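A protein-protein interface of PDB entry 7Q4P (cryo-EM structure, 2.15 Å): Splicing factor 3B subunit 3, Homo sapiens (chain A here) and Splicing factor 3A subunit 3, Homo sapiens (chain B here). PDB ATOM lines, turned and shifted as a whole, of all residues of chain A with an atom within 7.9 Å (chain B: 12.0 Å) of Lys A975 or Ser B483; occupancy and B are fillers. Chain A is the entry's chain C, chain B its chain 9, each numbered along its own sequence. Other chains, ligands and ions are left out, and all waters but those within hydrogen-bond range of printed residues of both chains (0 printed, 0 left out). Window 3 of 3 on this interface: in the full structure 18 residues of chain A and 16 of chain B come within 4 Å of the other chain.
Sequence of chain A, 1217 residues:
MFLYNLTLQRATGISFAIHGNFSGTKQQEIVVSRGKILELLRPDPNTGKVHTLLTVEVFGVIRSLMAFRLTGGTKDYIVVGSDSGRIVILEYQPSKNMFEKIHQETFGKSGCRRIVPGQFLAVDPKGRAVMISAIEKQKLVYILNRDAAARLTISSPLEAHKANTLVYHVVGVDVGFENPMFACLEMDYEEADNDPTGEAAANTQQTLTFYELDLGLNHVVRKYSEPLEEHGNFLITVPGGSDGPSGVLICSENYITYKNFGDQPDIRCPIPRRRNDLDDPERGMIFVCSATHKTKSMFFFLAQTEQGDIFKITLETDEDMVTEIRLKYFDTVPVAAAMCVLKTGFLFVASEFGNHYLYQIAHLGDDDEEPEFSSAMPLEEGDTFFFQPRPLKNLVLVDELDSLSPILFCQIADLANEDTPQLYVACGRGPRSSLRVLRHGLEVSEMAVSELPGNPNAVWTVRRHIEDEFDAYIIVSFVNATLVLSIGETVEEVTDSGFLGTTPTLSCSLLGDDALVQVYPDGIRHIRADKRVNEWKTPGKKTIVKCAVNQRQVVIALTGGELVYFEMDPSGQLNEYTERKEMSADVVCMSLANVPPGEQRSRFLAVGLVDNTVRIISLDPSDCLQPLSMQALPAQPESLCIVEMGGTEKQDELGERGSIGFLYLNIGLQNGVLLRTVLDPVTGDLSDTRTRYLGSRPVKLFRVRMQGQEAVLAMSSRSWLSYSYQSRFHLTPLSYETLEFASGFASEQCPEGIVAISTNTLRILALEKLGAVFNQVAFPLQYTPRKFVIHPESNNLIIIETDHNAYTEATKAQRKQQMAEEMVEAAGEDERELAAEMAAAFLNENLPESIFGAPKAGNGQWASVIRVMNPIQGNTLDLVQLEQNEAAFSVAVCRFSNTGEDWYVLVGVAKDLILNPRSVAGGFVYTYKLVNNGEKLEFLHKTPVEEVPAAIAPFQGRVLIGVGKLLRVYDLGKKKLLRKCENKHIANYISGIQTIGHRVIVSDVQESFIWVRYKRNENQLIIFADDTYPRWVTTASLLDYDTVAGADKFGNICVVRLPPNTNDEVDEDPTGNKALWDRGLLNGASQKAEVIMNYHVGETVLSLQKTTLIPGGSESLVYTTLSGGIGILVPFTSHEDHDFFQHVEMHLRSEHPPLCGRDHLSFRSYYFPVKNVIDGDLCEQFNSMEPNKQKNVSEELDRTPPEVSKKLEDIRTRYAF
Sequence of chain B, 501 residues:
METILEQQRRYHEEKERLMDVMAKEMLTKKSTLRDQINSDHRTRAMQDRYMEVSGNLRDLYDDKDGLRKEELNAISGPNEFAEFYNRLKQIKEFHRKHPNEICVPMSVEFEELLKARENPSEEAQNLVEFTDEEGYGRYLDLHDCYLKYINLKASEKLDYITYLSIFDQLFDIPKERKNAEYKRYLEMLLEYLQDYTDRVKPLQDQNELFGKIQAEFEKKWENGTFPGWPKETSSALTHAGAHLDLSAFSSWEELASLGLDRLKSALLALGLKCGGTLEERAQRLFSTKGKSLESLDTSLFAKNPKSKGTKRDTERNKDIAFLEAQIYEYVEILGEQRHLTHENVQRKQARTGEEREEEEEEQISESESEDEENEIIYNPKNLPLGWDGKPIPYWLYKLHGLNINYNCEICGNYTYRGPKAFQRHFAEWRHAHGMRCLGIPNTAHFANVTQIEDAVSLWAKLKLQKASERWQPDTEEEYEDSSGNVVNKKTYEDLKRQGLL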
ATOM      1  N   VAL A 925     -21.891  -5.078  24.842  1.00  0.00           N
ATOM      2  CA  VAL A 925     -21.454  -5.306  26.190  1.00  0.00           C
ATOM      3  C   VAL A 925     -20.195  -6.137  26.107  1.00  0.00           C
ATOM      4  O   VAL A 925     -20.239  -7.246  25.612  1.00  0.00           O
ATOM      5  CB  VAL A 925     -22.535  -5.987  27.049  1.00  0.00           C
ATOM      6  CG1 VAL A 925     -22.002  -6.134  28.482  1.00  0.00           C
ATOM      7  CG2 VAL A 925     -23.786  -5.115  27.002  1.00  0.00           C
ATOM      8  N   THR A 927     -17.439  -8.481  28.033  1.00  0.00           N
ATOM      9  CA  THR A 927     -17.390  -9.174  29.306  1.00  0.00           C
ATOM     10  C   THR A 927     -15.946  -9.550  29.542  1.00  0.00           C
ATOM     11  O   THR A 927     -15.296 -10.099  28.655  1.00  0.00           O
ATOM     12  CB  THR A 927     -18.250 -10.433  29.251  1.00  0.00           C
ATOM     13  OG1 THR A 927     -19.576  -9.956  29.087  1.00  0.00           O
ATOM     14  CG2 THR A 927     -18.236 -11.254  30.523  1.00  0.00           C
ATOM     15  N   LEU A 940     -13.515 -12.065  27.584  1.00  0.00           N
ATOM     16  CA  LEU A 940     -14.288 -13.254  27.354  1.00  0.00           C
ATOM     17  C   LEU A 940     -15.003 -13.133  26.020  1.00  0.00           C
ATOM     18  O   LEU A 940     -14.729 -13.902  25.113  1.00  0.00           O
ATOM     19  CB  LEU A 940     -15.276 -13.347  28.502  1.00  0.00           C
ATOM     20  CG  LEU A 940     -15.681 -14.757  28.866  1.00  0.00           C
ATOM     21  CD1 LEU A 940     -14.511 -15.370  29.620  1.00  0.00           C
ATOM     22  CD2 LEU A 940     -16.917 -14.719  29.756  1.00  0.00           C
ATOM     23  N   HIS A 941     -15.926 -12.185  25.916  1.00  0.00           N
ATOM     24  CA  HIS A 941     -16.733 -12.075  24.715  1.00  0.00           C
ATOM     25  C   HIS A 941     -17.337 -10.692  24.675  1.00  0.00           C
ATOM     26  O   HIS A 941     -17.371  -9.973  25.657  1.00  0.00           O
ATOM     27  CB  HIS A 941     -17.808 -13.148  24.506  1.00  0.00           C
ATOM     28  CG  HIS A 941     -18.609 -13.476  25.713  1.00  0.00           C
ATOM     29  ND1 HIS A 941     -19.519 -12.594  26.308  1.00  0.00           N
ATOM     30  CD2 HIS A 941     -18.583 -14.586  26.473  1.00  0.00           C
ATOM     31  CE1 HIS A 941     -19.964 -13.147  27.418  1.00  0.00           C
ATOM     32  NE2 HIS A 941     -19.487 -14.406  27.474  1.00  0.00           N
ATOM     33  N   LYS A 942     -17.810 -10.381  23.492  1.00  0.00           N
ATOM     34  CA  LYS A 942     -18.440  -9.134  23.178  1.00  0.00           C
ATOM     35  C   LYS A 942     -19.807  -9.439  22.596  1.00  0.00           C
ATOM     36  O   LYS A 942     -19.928 -10.192  21.642  1.00  0.00           O
ATOM     37  CB  LYS A 942     -17.552  -8.610  22.075  1.00  0.00           C
ATOM     38  CG  LYS A 942     -17.669  -7.137  21.891  1.00  0.00           C
ATOM     39  CD  LYS A 942     -16.660  -6.717  20.874  1.00  0.00           C
ATOM     40  CE  LYS A 942     -17.000  -5.348  20.360  1.00  0.00           C
ATOM     41  NZ  LYS A 942     -16.005  -4.842  19.387  1.00  0.00           N
ATOM     42  N   THR A 943     -20.831  -8.962  23.281  1.00  0.00           N
ATOM     43  CA  THR A 943     -22.199  -9.242  22.911  1.00  0.00           C
ATOM     44  C   THR A 943     -22.791  -7.969  22.323  1.00  0.00           C
ATOM     45  O   THR A 943     -22.806  -6.942  22.999  1.00  0.00           O
ATOM     46  CB  THR A 943     -22.970  -9.597  24.178  1.00  0.00           C
ATOM     47  OG1 THR A 943     -22.303 -10.618  24.921  1.00  0.00           O
ATOM     48  CG2 THR A 943     -24.388 -10.005  23.883  1.00  0.00           C
ATOM     49  N   PRO A 944     -23.228  -7.972  21.044  1.00  0.00           N
ATOM     50  CA  PRO A 944     -23.895  -6.808  20.452  1.00  0.00           C
ATOM     51  C   PRO A 944     -25.315  -6.559  20.960  1.00  0.00           C
ATOM     52  O   PRO A 944     -26.057  -7.488  21.253  1.00  0.00           O
ATOM     53  CB  PRO A 944     -23.916  -7.141  18.958  1.00  0.00           C
ATOM     54  CG  PRO A 944     -23.927  -8.656  18.925  1.00  0.00           C
ATOM     55  CD  PRO A 944     -23.049  -9.077  20.086  1.00  0.00           C
ATOM     56  N   LEU A 972     -24.961 -15.286  31.858  1.00  0.00           N
ATOM     57  CA  LEU A 972     -23.624 -15.264  31.285  1.00  0.00           C
ATOM     58  C   LEU A 972     -23.473 -16.060  29.988  1.00  0.00           C
ATOM     59  O   LEU A 972     -23.055 -15.485  28.987  1.00  0.00           O
ATOM     60  CB  LEU A 972     -22.522 -15.507  32.323  1.00  0.00           C
ATOM     61  CG  LEU A 972     -21.085 -15.452  31.807  1.00  0.00           C
ATOM     62  CD1 LEU A 972     -20.624 -14.022  31.500  1.00  0.00           C
ATOM     63  CD2 LEU A 972     -20.189 -16.042  32.868  1.00  0.00           C
ATOM     64  N   GLY A 973     -23.691 -17.368  29.958  1.00  0.00           N
ATOM     65  CA  GLY A 973     -23.384 -17.974  28.654  1.00  0.00           C
ATOM     66  C   GLY A 973     -21.880 -18.218  28.416  1.00  0.00           C
ATOM     67  O   GLY A 973     -21.103 -18.113  29.364  1.00  0.00           O
ATOM     68  N   LYS A 974     -21.461 -18.536  27.161  1.00  0.00           N
ATOM     69  CA  LYS A 974     -20.106 -18.975  26.830  1.00  0.00           C
ATOM     70  C   LYS A 974     -19.535 -18.098  25.724  1.00  0.00           C
ATOM     71  O   LYS A 974     -18.434 -17.570  25.850  1.00  0.00           O
ATOM     72  CB  LYS A 974     -20.090 -20.430  26.354  1.00  0.00           C
ATOM     73  CG  LYS A 974     -20.491 -21.452  27.405  1.00  0.00           C
ATOM     74  CD  LYS A 974     -19.334 -22.039  28.195  1.00  0.00           C
ATOM     75  CE  LYS A 974     -19.069 -21.337  29.511  1.00  0.00           C
ATOM     76  NZ  LYS A 974     -17.950 -21.965  30.252  1.00  0.00           N
ATOM     77  N   LYS A 975     -20.389 -17.788  24.746  1.00  0.00           N
ATOM     78  CA  LYS A 975     -20.028 -16.945  23.621  1.00  0.00           C
ATOM     79  C   LYS A 975     -20.695 -15.569  23.723  1.00  0.00           C
ATOM     80  O   LYS A 975     -20.341 -14.661  22.980  1.00  0.00           O
ATOM     81  CB  LYS A 975     -20.341 -17.671  22.307  1.00  0.00           C
ATOM     82  CG  LYS A 975     -19.474 -18.891  22.014  1.00  0.00           C
ATOM     83  CD  LYS A 975     -19.265 -19.117  20.529  1.00  0.00           C
ATOM     84  CE  LYS A 975     -17.892 -19.657  20.182  1.00  0.00           C
ATOM     85  NZ  LYS A 975     -17.715 -21.067  20.602  1.00  0.00           N
ATOM     86  N   LYS A 976     -21.712 -15.400  24.565  1.00  0.00           N
ATOM     87  CA  LYS A 976     -22.456 -14.152  24.540  1.00  0.00           C
ATOM     88  C   LYS A 976     -23.091 -14.023  25.906  1.00  0.00           C
ATOM     89  O   LYS A 976     -23.339 -15.034  26.544  1.00  0.00           O
ATOM     90  CB  LYS A 976     -23.606 -14.332  23.542  1.00  0.00           C
ATOM     91  CG  LYS A 976     -23.402 -13.653  22.196  1.00  0.00           C
ATOM     92  CD  LYS A 976     -24.659 -13.047  21.621  1.00  0.00           C
ATOM     93  CE  LYS A 976     -25.865 -13.949  21.768  1.00  0.00           C
ATOM     94  NZ  LYS A 976     -27.064 -13.360  21.138  1.00  0.00           N
ATOM     95  N   LEU A 977     -23.572 -12.840  26.265  1.00  0.00           N
ATOM     96  CA  LEU A 977     -24.546 -12.789  27.335  1.00  0.00           C
ATOM     97  C   LEU A 977     -25.907 -13.174  26.770  1.00  0.00           C
ATOM     98  O   LEU A 977     -26.326 -12.681  25.743  1.00  0.00           O
ATOM     99  CB  LEU A 977     -24.562 -11.353  27.834  1.00  0.00           C
ATOM    100  CG  LEU A 977     -23.320 -10.921  28.599  1.00  0.00           C
ATOM    101  CD1 LEU A 977     -23.431  -9.435  28.831  1.00  0.00           C
ATOM    102  CD2 LEU A 977     -23.201 -11.632  29.945  1.00  0.00           C
ATOM    103  N   LEU A 978     -26.648 -14.016  27.462  1.00  0.00           N
ATOM    104  CA  LEU A 978     -27.930 -14.489  26.963  1.00  0.00           C
ATOM    105  C   LEU A 978     -29.092 -13.713  27.581  1.00  0.00           C
ATOM    106  O   LEU A 978     -29.271 -13.725  28.808  1.00  0.00           O
ATOM    107  CB  LEU A 978     -28.001 -15.956  27.373  1.00  0.00           C
ATOM    108  CG  LEU A 978     -26.849 -16.825  26.879  1.00  0.00           C
ATOM    109  CD1 LEU A 978     -26.915 -18.204  27.531  1.00  0.00           C
ATOM    110  CD2 LEU A 978     -26.899 -16.976  25.365  1.00  0.00           C
ATOM    111  N   GLU B 478     -32.999 -16.535  25.041  1.00  0.00           N
ATOM    112  CA  GLU B 478     -31.804 -17.010  24.379  1.00  0.00           C
ATOM    113  C   GLU B 478     -31.231 -18.091  25.271  1.00  0.00           C
ATOM    114  O   GLU B 478     -31.199 -17.939  26.488  1.00  0.00           O
ATOM    115  CB  GLU B 478     -30.789 -15.879  24.228  1.00  0.00           C
ATOM    116  CG  GLU B 478     -31.202 -14.804  23.238  1.00  0.00           C
ATOM    117  CD  GLU B 478     -30.175 -13.729  22.933  1.00  0.00           C
ATOM    118  OE1 GLU B 478     -29.507 -13.258  23.878  1.00  0.00           O
ATOM    119  OE2 GLU B 478     -30.047 -13.367  21.744  1.00  0.00           O
ATOM    120  N   TYR B 479     -30.881 -19.211  24.647  1.00  0.00           N
ATOM    121  CA  TYR B 479     -30.354 -20.372  25.335  1.00  0.00           C
ATOM    122  C   TYR B 479     -29.070 -20.828  24.651  1.00  0.00           C
ATOM    123  O   TYR B 479     -28.830 -20.497  23.496  1.00  0.00           O
ATOM    124  CB  TYR B 479     -31.412 -21.472  25.296  1.00  0.00           C
ATOM    125  CG  TYR B 479     -32.508 -21.321  26.316  1.00  0.00           C
ATOM    126  CD1 TYR B 479     -33.725 -20.708  26.018  1.00  0.00           C
ATOM    127  CD2 TYR B 479     -32.319 -21.815  27.598  1.00  0.00           C
ATOM    128  CE1 TYR B 479     -34.726 -20.603  26.979  1.00  0.00           C
ATOM    129  CE2 TYR B 479     -33.312 -21.725  28.559  1.00  0.00           C
ATOM    130  CZ  TYR B 479     -34.520 -21.123  28.251  1.00  0.00           C
ATOM    131  OH  TYR B 479     -35.464 -21.069  29.238  1.00  0.00           O
ATOM    132  N   GLU B 480     -28.261 -21.610  25.361  1.00  0.00           N
ATOM    133  CA  GLU B 480     -27.081 -22.191  24.740  1.00  0.00           C
ATOM    134  C   GLU B 480     -27.147 -23.717  24.816  1.00  0.00           C
ATOM    135  O   GLU B 480     -27.446 -24.269  25.874  1.00  0.00           O
ATOM    136  CB  GLU B 480     -25.840 -21.628  25.420  1.00  0.00           C
ATOM    137  CG  GLU B 480     -25.222 -20.436  24.708  1.00  0.00           C
ATOM    138  CD  GLU B 480     -24.028 -19.817  25.410  1.00  0.00           C
ATOM    139  OE1 GLU B 480     -23.553 -18.736  24.968  1.00  0.00           O
ATOM    140  OE2 GLU B 480     -23.558 -20.417  26.403  1.00  0.00           O
ATOM    141  N   ASP B 481     -26.848 -24.397  23.697  1.00  0.00           N
ATOM    142  CA  ASP B 481     -26.876 -25.852  23.646  1.00  0.00           C
ATOM    143  C   ASP B 481     -25.509 -26.414  24.034  1.00  0.00           C
ATOM    144  O   ASP B 481     -25.379 -27.044  25.084  1.00  0.00           O
ATOM    145  CB  ASP B 481     -27.457 -26.372  22.326  1.00  0.00           C
ATOM    146  CG  ASP B 481     -26.775 -25.839  21.075  1.00  0.00           C
ATOM    147  OD1 ASP B 481     -25.687 -26.344  20.736  1.00  0.00           O
ATOM    148  OD2 ASP B 481     -27.333 -24.914  20.456  1.00  0.00           O
ATOM    149  N   SER B 482     -24.504 -26.170  23.182  1.00  0.00           N
ATOM    150  CA  SER B 482     -23.141 -26.648  23.366  1.00  0.00           C
ATOM    151  C   SER B 482     -22.172 -25.768  22.578  1.00  0.00           C
ATOM    152  O   SER B 482     -22.451 -25.410  21.434  1.00  0.00           O
ATOM    153  CB  SER B 482     -23.005 -28.102  22.971  1.00  0.00           C
ATOM    154  OG  SER B 482     -23.376 -28.299  21.615  1.00  0.00           O
ATOM    155  N   SER B 483     -21.042 -25.436  23.223  1.00  0.00           N
ATOM    156  CA  SER B 483     -19.962 -24.621  22.678  1.00  0.00           C
ATOM    157  C   SER B 483     -20.440 -23.209  22.326  1.00  0.00           C
ATOM    158  O   SER B 483     -19.870 -22.556  21.452  1.00  0.00           O
ATOM    159  CB  SER B 483     -19.262 -25.310  21.522  1.00  0.00           C
ATOM    160  OG  SER B 483     -18.668 -26.529  21.944  1.00  0.00           O
ATOM    161  N   GLY B 484     -21.481 -22.749  23.032  1.00  0.00           N
ATOM    162  CA  GLY B 484     -21.994 -21.393  22.920  1.00  0.00           C
ATOM    163  C   GLY B 484     -22.734 -21.143  21.605  1.00  0.00           C
ATOM    164  O   GLY B 484     -22.449 -20.169  20.912  1.00  0.00           O
ATOM    165  N   ASN B 485     -23.683 -22.033  21.282  1.00  0.00           N
ATOM    166  CA  ASN B 485     -24.555 -21.879  20.126  1.00  0.00           C
ATOM    167  C   ASN B 485     -25.908 -21.346  20.591  1.00  0.00           C
ATOM    168  O   ASN B 485     -26.602 -21.984  21.377  1.00  0.00           O
ATOM    169  CB  ASN B 485     -24.663 -23.171  19.312  1.00  0.00           C
ATOM    170  CG  ASN B 485     -23.383 -23.540  18.589  1.00  0.00           C
ATOM    171  OD1 ASN B 485     -22.809 -22.727  17.867  1.00  0.00           O
ATOM    172  ND2 ASN B 485     -22.936 -24.774  18.763  1.00  0.00           N
ATOM    173  N   VAL B 486     -26.280 -20.158  20.104  1.00  0.00           N
ATOM    174  CA  VAL B 486     -27.468 -19.473  20.610  1.00  0.00           C
ATOM    175  C   VAL B 486     -28.727 -20.043  19.949  1.00  0.00           C
ATOM    176  O   VAL B 486     -28.826 -20.106  18.724  1.00  0.00           O
ATOM    177  CB  VAL B 486     -27.358 -17.935  20.517  1.00  0.00           C
ATOM    178  CG1 VAL B 486     -28.618 -17.201  20.978  1.00  0.00           C
ATOM    179  CG2 VAL B 486     -26.141 -17.400  21.263  1.00  0.00           C
ATOM    180  N   VAL B 487     -29.664 -20.489  20.799  1.00  0.00           N
ATOM    181  CA  VAL B 487     -30.882 -21.174  20.389  1.00  0.00           C
ATOM    182  C   VAL B 487     -32.066 -20.658  21.200  1.00  0.00           C
ATOM    183  O   VAL B 487     -31.878 -20.131  22.288  1.00  0.00           O
ATOM    184  CB  VAL B 487     -30.759 -22.706  20.514  1.00  0.00           C
ATOM    185  CG1 VAL B 487     -30.018 -23.305  19.336  1.00  0.00           C
ATOM    186  CG2 VAL B 487     -30.212 -23.198  21.852  1.00  0.00           C
ATOM    187  N   TYR B 492     -34.068 -25.622  22.301  1.00  0.00           N
ATOM    188  CA  TYR B 492     -33.360 -26.043  23.499  1.00  0.00           C
ATOM    189  C   TYR B 492     -33.928 -27.369  24.015  1.00  0.00           C
ATOM    190  O   TYR B 492     -33.171 -28.310  24.256  1.00  0.00           O
ATOM    191  CB  TYR B 492     -33.454 -24.962  24.574  1.00  0.00           C
ATOM    192  CG  TYR B 492     -32.574 -25.183  25.774  1.00  0.00           C
ATOM    193  CD1 TYR B 492     -31.191 -25.190  25.657  1.00  0.00           C
ATOM    194  CD2 TYR B 492     -33.124 -25.368  27.035  1.00  0.00           C
ATOM    195  CE1 TYR B 492     -30.376 -25.348  26.771  1.00  0.00           C
ATOM    196  CE2 TYR B 492     -32.323 -25.545  28.153  1.00  0.00           C
ATOM    197  CZ  TYR B 492     -30.945 -25.533  28.022  1.00  0.00           C
ATOM    198  OH  TYR B 492     -30.160 -25.722  29.125  1.00  0.00           O
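The side-chain amino group of Lys A975 sits at hydrogen-bond distance from the backbone carbonyl oxygen of Ser B483 (2.8 Å).
The side-chain carboxylate of Glu B480 sits at hydrogen-bond distance from the backbone NH of Lys A974, 2.9 Å away.
OE2 of Glu B478 lies within salt-bridge range of NZ of Lys A976, at 3.0 Å.
The side-chain carboxylate (OE1) of Glu B480 lies within hydrogen-bond range of the backbone NH (N) of Lys A975, at 3.3 Å.
The side-chain hydroxyl (OG1) of Thr A943 is in hydrogen-bond range of the backbone NH (N) of Leu A977 (2.9 Å).
Among the printed residues, merely in contact across the chains: Gly A973 with Glu B480, Lys A975 with Gly B484, Lys A976 with Val B486, Leu A978 with Glu B478, Leu A977 with Glu B478, Leu A978 with Glu B480 and Lys A976 with Glu B480.
Of chain B, only Glu B480 (3.3 Å), Ser B483 (2.8 Å) and Gly B484 (3.4 Å) come within 4 Å of Lys A975.
Printed residues of chain A within 4 Å of Ser B483: Lys A975.
No residue of chain B comes within 4 Å of His A941.
Printed residues of chain B within 4 Å of Gly A973: Glu B480 (3.3 Å).
Lys A974 touches one residue of chain B.
Lys A976 touches three residues of chain B.
Of chain A, only Lys A975 (3.4 Å) comes within 4 Å of Gly B484.
Of the printed residues of chain A, Val B486 touches Lys A976.
Of the printed residues of chain A, Glu B480 touches Gly A973, Lys A974, Lys A975, Lys A976 and Leu A978.
Ser B482 touches none of the printed residues of chain A.
The nearest residue of chain B that does not touch Lys A975 is Asn B485 (5.3 Å).
The nearest printed residue of chain A that does not touch Glu B480 is Leu A972 (5.2 Å).
Hydrophobic or aromatic side chains of chain B within 4 Å of the printed part of chain A: Val B486.
Of the 14 printed residues of chain A, 6 touch a printed residue of chain B.
Printed residues of chain A that touch a printed residue of chain B: Gly A973, Lys A974, Lys A975, Lys A976, Leu A977 and Leu A978.
Hydrophobic or aromatic side chains of chain A within 4 Å of the printed part of chain B: Leu A978.
Along chain A the printed residues that touch a printed residue of chain B span positions 973 to 978.
Among the printed residues, 11 pairs touch across the chains.
Among the printed residues, Asp or Glu carboxylates within 4 Å of a Lys or Arg side-chain nitrogen of the other chain: Lys A976 with Glu B478 (3.0 Å).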
